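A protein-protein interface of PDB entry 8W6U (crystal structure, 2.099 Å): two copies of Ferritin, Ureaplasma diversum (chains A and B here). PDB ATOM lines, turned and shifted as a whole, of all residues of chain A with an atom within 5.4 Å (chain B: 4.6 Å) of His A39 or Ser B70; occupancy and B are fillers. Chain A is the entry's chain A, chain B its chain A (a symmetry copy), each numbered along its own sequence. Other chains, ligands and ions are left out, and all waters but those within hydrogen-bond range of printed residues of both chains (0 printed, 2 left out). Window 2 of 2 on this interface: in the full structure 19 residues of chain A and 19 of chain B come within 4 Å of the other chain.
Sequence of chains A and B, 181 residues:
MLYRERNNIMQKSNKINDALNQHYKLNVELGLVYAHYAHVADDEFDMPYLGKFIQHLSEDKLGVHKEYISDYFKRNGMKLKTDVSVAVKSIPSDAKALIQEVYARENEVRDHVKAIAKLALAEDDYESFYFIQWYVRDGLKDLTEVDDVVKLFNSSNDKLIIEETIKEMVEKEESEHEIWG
The side-chain hydroxyl of Ser B70 sits at hydrogen-bond distance from a ring nitrogen (ND1) of His A39, 2.6 Å away. The backbone carbonyl oxygen of Leu B80 lies within hydrogen-bond range of a ring nitrogen (NE2) of His A36 (3.3 Å). The side-chain carboxylate (OD2) of Asp A42 is in salt-bridge range of the side-chain amino group (NZ) of Lys B74 (2.9 Å).
Among the printed residues, pairs that only touch across the chains: His A39 with Lys B74, Asp A43 with Lys B74, His A39 with Leu B80 and His A39 with Phe B73.
Of the printed residues of chain B, His A36 touches Leu B80. Ser B70 touches one residue of chain A. Printed residues of chain A within 4 Å of Phe B73: His A39. The nearest printed residue of chain A that does not touch Ser B70 is Ala A35 (5.4 Å). The nearest printed residue of chain A that does not touch Phe B73 is Asp A43 (4.6 Å).
Hydrophobic or aromatic side chains of chain A within 4 Å of the printed part of chain B: His A36 and His A39. Of the 10 printed residues of chain B, 4 touch a printed residue of chain A. Printed residues of chain B that touch a printed residue of chain A: Ser B70, Phe B73, Lys B74 and Leu B80. Among the printed residues, 7 pairs touch across the chains.
No position is printed for both chains. Of the 7 pairs that touch across the chains among the printed residues, none has its exchanged pair printed and touching as well.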
ATOM      1  N   TYR A  34     -23.557  16.614  21.460  1.00  0.00           N
ATOM      2  CA  TYR A  34     -23.912  17.743  20.607  1.00  0.00           C
ATOM      3  C   TYR A  34     -23.562  17.462  19.148  1.00  0.00           C
ATOM      4  O   TYR A  34     -24.314  17.841  18.244  1.00  0.00           O
ATOM      5  CB  TYR A  34     -23.216  19.012  21.104  1.00  0.00           C
ATOM      6  CG  TYR A  34     -23.764  19.574  22.393  1.00  0.00           C
ATOM      7  CD1 TYR A  34     -24.947  19.101  22.939  1.00  0.00           C
ATOM      8  CD2 TYR A  34     -23.102  20.596  23.054  1.00  0.00           C
ATOM      9  CE1 TYR A  34     -25.448  19.618  24.120  1.00  0.00           C
ATOM     10  CE2 TYR A  34     -23.601  21.127  24.228  1.00  0.00           C
ATOM     11  CZ  TYR A  34     -24.778  20.640  24.754  1.00  0.00           C
ATOM     12  OH  TYR A  34     -25.267  21.164  25.932  1.00  0.00           O
ATOM     13  N   ALA A  35     -22.432  16.789  18.897  1.00  0.00           N
ATOM     14  CA  ALA A  35     -22.099  16.419  17.525  1.00  0.00           C
ATOM     15  C   ALA A  35     -23.193  15.543  16.921  1.00  0.00           C
ATOM     16  O   ALA A  35     -23.570  15.716  15.757  1.00  0.00           O
ATOM     17  CB  ALA A  35     -20.748  15.699  17.468  1.00  0.00           C
ATOM     18  N   HIS A  36     -23.722  14.604  17.706  1.00  0.00           N
ATOM     19  CA  HIS A  36     -24.837  13.786  17.238  1.00  0.00           C
ATOM     20  C   HIS A  36     -26.079  14.638  17.013  1.00  0.00           C
ATOM     21  O   HIS A  36     -26.718  14.551  15.959  1.00  0.00           O
ATOM     22  CB  HIS A  36     -25.125  12.675  18.240  1.00  0.00           C
ATOM     23  CG  HIS A  36     -25.896  11.528  17.664  1.00  0.00           C
ATOM     24  ND1 HIS A  36     -27.231  11.616  17.335  1.00  0.00           N
ATOM     25  CD2 HIS A  36     -25.521  10.259  17.380  1.00  0.00           C
ATOM     26  CE1 HIS A  36     -27.641  10.457  16.849  1.00  0.00           C
ATOM     27  NE2 HIS A  36     -26.621   9.616  16.864  1.00  0.00           N
ATOM     28  N   TYR A  37     -26.424  15.478  17.995  1.00  0.00           N
ATOM     29  CA  TYR A  37     -27.583  16.364  17.863  1.00  0.00           C
ATOM     30  C   TYR A  37     -27.462  17.283  16.653  1.00  0.00           C
ATOM     31  O   TYR A  37     -28.471  17.613  16.020  1.00  0.00           O
ATOM     32  CB  TYR A  37     -27.756  17.203  19.127  1.00  0.00           C
ATOM     33  CG  TYR A  37     -28.310  16.467  20.331  1.00  0.00           C
ATOM     34  CD1 TYR A  37     -28.512  15.087  20.319  1.00  0.00           C
ATOM     35  CD2 TYR A  37     -28.613  17.163  21.496  1.00  0.00           C
ATOM     36  CE1 TYR A  37     -29.023  14.427  21.453  1.00  0.00           C
ATOM     37  CE2 TYR A  37     -29.106  16.526  22.610  1.00  0.00           C
ATOM     38  CZ  TYR A  37     -29.315  15.165  22.591  1.00  0.00           C
ATOM     39  OH  TYR A  37     -29.802  14.577  23.730  1.00  0.00           O
ATOM     40  N   ALA A  38     -26.242  17.735  16.330  1.00  0.00           N
ATOM     41  CA  ALA A  38     -26.059  18.559  15.134  1.00  0.00           C
ATOM     42  C   ALA A  38     -26.366  17.771  13.868  1.00  0.00           C
ATOM     43  O   ALA A  38     -27.007  18.285  12.943  1.00  0.00           O
ATOM     44  CB  ALA A  38     -24.635  19.110  15.069  1.00  0.00           C
ATOM     45  N   HIS A  39     -25.898  16.525  13.802  1.00  0.00           N
ATOM     46  CA  HIS A  39     -26.253  15.652  12.691  1.00  0.00           C
ATOM     47  C   HIS A  39     -27.771  15.529  12.544  1.00  0.00           C
ATOM     48  O   HIS A  39     -28.331  15.754  11.463  1.00  0.00           O
ATOM     49  CB  HIS A  39     -25.627  14.273  12.899  1.00  0.00           C
ATOM     50  CG  HIS A  39     -25.976  13.301  11.822  1.00  0.00           C
ATOM     51  ND1 HIS A  39     -25.191  13.116  10.705  1.00  0.00           N
ATOM     52  CD2 HIS A  39     -27.061  12.509  11.658  1.00  0.00           C
ATOM     53  CE1 HIS A  39     -25.762  12.225   9.913  1.00  0.00           C
ATOM     54  NE2 HIS A  39     -26.898  11.844  10.468  1.00  0.00           N
ATOM     55  N   VAL A  40     -28.450  15.170  13.636  1.00  0.00           N
ATOM     56  CA  VAL A  40     -29.904  14.984  13.621  1.00  0.00           C
ATOM     57  C   VAL A  40     -30.639  16.273  13.238  1.00  0.00           C
ATOM     58  O   VAL A  40     -31.630  16.241  12.491  1.00  0.00           O
ATOM     59  CB  VAL A  40     -30.355  14.457  14.995  1.00  0.00           C
ATOM     60  CG1 VAL A  40     -31.859  14.363  15.075  1.00  0.00           C
ATOM     61  CG2 VAL A  40     -29.725  13.094  15.240  1.00  0.00           C
ATOM     62  N   ALA A  41     -30.207  17.416  13.785  1.00  0.00           N
ATOM     63  CA  ALA A  41     -30.834  18.695  13.456  1.00  0.00           C
ATOM     64  C   ALA A  41     -30.889  18.903  11.946  1.00  0.00           C
ATOM     65  O   ALA A  41     -31.925  19.272  11.378  1.00  0.00           O
ATOM     66  CB  ALA A  41     -30.058  19.838  14.116  1.00  0.00           C
ATOM     67  N   ASP A  42     -29.768  18.655  11.281  1.00  0.00           N
ATOM     68  CA  ASP A  42     -29.712  18.761   9.832  1.00  0.00           C
ATOM     69  C   ASP A  42     -30.448  17.602   9.181  1.00  0.00           C
ATOM     70  O   ASP A  42     -31.380  17.796   8.393  1.00  0.00           O
ATOM     71  CB  ASP A  42     -28.245  18.798   9.389  1.00  0.00           C
ATOM     72  CG  ASP A  42     -28.077  19.114   7.921  1.00  0.00           C
ATOM     73  OD1 ASP A  42     -29.090  19.222   7.200  1.00  0.00           O
ATOM     74  OD2 ASP A  42     -26.917  19.252   7.493  1.00  0.00           O
ATOM     75  N   ASP A  43     -30.057  16.380   9.527  1.00  0.00           N
ATOM     76  CA  ASP A  43     -30.475  15.226   8.745  1.00  0.00           C
ATOM     77  C   ASP A  43     -31.950  14.910   8.965  1.00  0.00           C
ATOM     78  O   ASP A  43     -32.724  14.809   8.006  1.00  0.00           O
ATOM     79  CB  ASP A  43     -29.593  14.032   9.103  1.00  0.00           C
ATOM     80  CG  ASP A  43     -29.963  12.790   8.336  1.00  0.00           C
ATOM     81  OD1 ASP A  43     -29.993  12.855   7.095  1.00  0.00           O
ATOM     82  OD2 ASP A  43     -30.234  11.756   8.987  1.00  0.00           O
ATOM     83  N   GLU A  44     -32.364  14.767  10.220  1.00  0.00           N
ATOM     84  CA  GLU A  44     -33.739  14.372  10.498  1.00  0.00           C
ATOM     85  C   GLU A  44     -34.711  15.552  10.504  1.00  0.00           C
ATOM     86  O   GLU A  44     -35.823  15.434   9.982  1.00  0.00           O
ATOM     87  CB  GLU A  44     -33.801  13.621  11.832  1.00  0.00           C
ATOM     88  CG  GLU A  44     -35.227  13.339  12.310  1.00  0.00           C
ATOM     89  CD  GLU A  44     -35.415  11.923  12.821  1.00  0.00           C
ATOM     90  OE1 GLU A  44     -34.889  11.599  13.911  1.00  0.00           O
ATOM     91  OE2 GLU A  44     -36.083  11.134  12.118  1.00  0.00           O
ATOM     92  N   LYS B  66     -14.145  12.288  11.541  1.00  0.00           N
ATOM     93  CA  LYS B  66     -15.507  11.991  11.933  1.00  0.00           C
ATOM     94  C   LYS B  66     -16.555  12.786  11.182  1.00  0.00           C
ATOM     95  O   LYS B  66     -17.602  12.273  10.862  1.00  0.00           O
ATOM     96  CB  LYS B  66     -15.669  12.112  13.436  1.00  0.00           C
ATOM     97  CG  LYS B  66     -16.053  13.456  14.026  1.00  0.00           C
ATOM     98  CD  LYS B  66     -16.247  13.338  15.522  1.00  0.00           C
ATOM     99  CE  LYS B  66     -17.066  14.482  16.082  1.00  0.00           C
ATOM    100  NZ  LYS B  66     -16.661  15.787  15.517  1.00  0.00           N
ATOM    101  N   GLU B  67     -16.256  14.028  10.880  1.00  0.00           N
ATOM    102  CA  GLU B  67     -17.182  14.863  10.181  1.00  0.00           C
ATOM    103  C   GLU B  67     -17.599  14.354   8.819  1.00  0.00           C
ATOM    104  O   GLU B  67     -18.748  14.391   8.491  1.00  0.00           O
ATOM    105  CB  GLU B  67     -16.637  16.274  10.095  1.00  0.00           C
ATOM    106  CG  GLU B  67     -16.794  17.065  11.395  1.00  0.00           C
ATOM    107  CD  GLU B  67     -18.191  16.989  12.010  1.00  0.00           C
ATOM    108  OE1 GLU B  67     -19.163  17.428  11.359  1.00  0.00           O
ATOM    109  OE2 GLU B  67     -18.319  16.513  13.160  1.00  0.00           O
ATOM    110  N   TYR B  68     -16.655  13.865   8.052  1.00  0.00           N
ATOM    111  CA  TYR B  68     -16.942  13.354   6.740  1.00  0.00           C
ATOM    112  C   TYR B  68     -17.876  12.146   6.765  1.00  0.00           C
ATOM    113  O   TYR B  68     -18.671  11.993   5.888  1.00  0.00           O
ATOM    114  CB  TYR B  68     -15.662  13.092   5.976  1.00  0.00           C
ATOM    115  CG  TYR B  68     -14.813  14.288   5.638  1.00  0.00           C
ATOM    116  CD1 TYR B  68     -15.349  15.559   5.562  1.00  0.00           C
ATOM    117  CD2 TYR B  68     -13.471  14.133   5.363  1.00  0.00           C
ATOM    118  CE1 TYR B  68     -14.568  16.643   5.239  1.00  0.00           C
ATOM    119  CE2 TYR B  68     -12.682  15.209   5.036  1.00  0.00           C
ATOM    120  CZ  TYR B  68     -13.236  16.460   4.977  1.00  0.00           C
ATOM    121  OH  TYR B  68     -12.450  17.526   4.653  1.00  0.00           O
ATOM    122  N   ILE B  69     -17.793  11.311   7.792  1.00  0.00           N
ATOM    123  CA  ILE B  69     -18.729  10.212   7.940  1.00  0.00           C
ATOM    124  C   ILE B  69     -20.143  10.712   8.207  1.00  0.00           C
ATOM    125  O   ILE B  69     -21.064  10.287   7.558  1.00  0.00           O
ATOM    126  CB  ILE B  69     -18.250   9.190   8.981  1.00  0.00           C
ATOM    127  CG1 ILE B  69     -16.998   8.474   8.477  1.00  0.00           C
ATOM    128  CG2 ILE B  69     -19.317   8.176   9.329  1.00  0.00           C
ATOM    129  CD1 ILE B  69     -16.196   7.794   9.557  1.00  0.00           C
ATOM    130  N   SER B  70     -20.295  11.649   9.129  1.00  0.00           N
ATOM    131  CA  SER B  70     -21.595  12.211   9.406  1.00  0.00           C
ATOM    132  C   SER B  70     -22.189  12.860   8.171  1.00  0.00           C
ATOM    133  O   SER B  70     -23.342  12.677   7.883  1.00  0.00           O
ATOM    134  CB  SER B  70     -21.545  13.198  10.570  1.00  0.00           C
ATOM    135  OG  SER B  70     -22.732  13.946  10.682  1.00  0.00           O
ATOM    136  N   ASP B  71     -21.382  13.584   7.430  1.00  0.00           N
ATOM    137  CA  ASP B  71     -21.837  14.220   6.217  1.00  0.00           C
ATOM    138  C   ASP B  71     -22.314  13.202   5.204  1.00  0.00           C
ATOM    139  O   ASP B  71     -23.360  13.373   4.632  1.00  0.00           O
ATOM    140  CB  ASP B  71     -20.730  15.090   5.655  1.00  0.00           C
ATOM    141  CG  ASP B  71     -21.129  15.833   4.434  1.00  0.00           C
ATOM    142  OD1 ASP B  71     -21.860  16.820   4.560  1.00  0.00           O
ATOM    143  OD2 ASP B  71     -20.689  15.440   3.352  1.00  0.00           O
ATOM    144  N   TYR B  72     -21.532  12.156   5.000  1.00  0.00           N
ATOM    145  CA  TYR B  72     -21.906  11.111   4.089  1.00  0.00           C
ATOM    146  C   TYR B  72     -23.229  10.472   4.443  1.00  0.00           C
ATOM    147  O   TYR B  72     -24.039  10.242   3.583  1.00  0.00           O
ATOM    148  CB  TYR B  72     -20.806  10.068   4.069  1.00  0.00           C
ATOM    149  CG  TYR B  72     -20.940   8.999   3.035  1.00  0.00           C
ATOM    150  CD1 TYR B  72     -21.228   9.316   1.727  1.00  0.00           C
ATOM    151  CD2 TYR B  72     -20.751   7.673   3.361  1.00  0.00           C
ATOM    152  CE1 TYR B  72     -21.344   8.343   0.774  1.00  0.00           C
ATOM    153  CE2 TYR B  72     -20.860   6.691   2.408  1.00  0.00           C
ATOM    154  CZ  TYR B  72     -21.154   7.042   1.118  1.00  0.00           C
ATOM    155  OH  TYR B  72     -21.282   6.101   0.162  1.00  0.00           O
ATOM    156  N   PHE B  73     -23.442  10.218   5.720  1.00  0.00           N
ATOM    157  CA  PHE B  73     -24.659   9.592   6.186  1.00  0.00           C
ATOM    158  C   PHE B  73     -25.884  10.438   5.862  1.00  0.00           C
ATOM    159  O   PHE B  73     -26.899   9.916   5.474  1.00  0.00           O
ATOM    160  CB  PHE B  73     -24.560   9.308   7.665  1.00  0.00           C
ATOM    161  CG  PHE B  73     -23.705   8.127   8.036  1.00  0.00           C
ATOM    162  CD1 PHE B  73     -22.982   7.419   7.102  1.00  0.00           C
ATOM    163  CD2 PHE B  73     -23.629   7.736   9.351  1.00  0.00           C
ATOM    164  CE1 PHE B  73     -22.214   6.343   7.477  1.00  0.00           C
ATOM    165  CE2 PHE B  73     -22.861   6.664   9.733  1.00  0.00           C
ATOM    166  CZ  PHE B  73     -22.158   5.962   8.794  1.00  0.00           C
ATOM    167  N   LYS B  74     -25.758  11.741   5.985  1.00  0.00           N
ATOM    168  CA  LYS B  74     -26.837  12.641   5.670  1.00  0.00           C
ATOM    169  C   LYS B  74     -27.232  12.591   4.233  1.00  0.00           C
ATOM    170  O   LYS B  74     -28.364  12.829   3.900  1.00  0.00           O
ATOM    171  CB  LYS B  74     -26.423  14.066   5.954  1.00  0.00           C
ATOM    172  CG  LYS B  74     -26.104  14.432   7.380  1.00  0.00           C
ATOM    173  CD  LYS B  74     -25.708  15.895   7.395  1.00  0.00           C
ATOM    174  CE  LYS B  74     -24.923  16.278   8.623  1.00  0.00           C
ATOM    175  NZ  LYS B  74     -24.678  17.738   8.589  1.00  0.00           N
ATOM    176  N   LEU B  80     -26.416   7.419  11.761  1.00  0.00           N
ATOM    177  CA  LEU B  80     -25.336   7.639  12.673  1.00  0.00           C
ATOM    178  C   LEU B  80     -25.586   7.107  14.040  1.00  0.00           C
ATOM    179  O   LEU B  80     -26.653   7.263  14.588  1.00  0.00           O
ATOM    180  CB  LEU B  80     -25.001   9.109  12.806  1.00  0.00           C
ATOM    181  CG  LEU B  80     -23.793   9.517  13.645  1.00  0.00           C
ATOM    182  CD1 LEU B  80     -22.497   9.065  13.000  1.00  0.00           C
ATOM    183  CD2 LEU B  80     -23.794  11.008  13.910  1.00  0.00           C
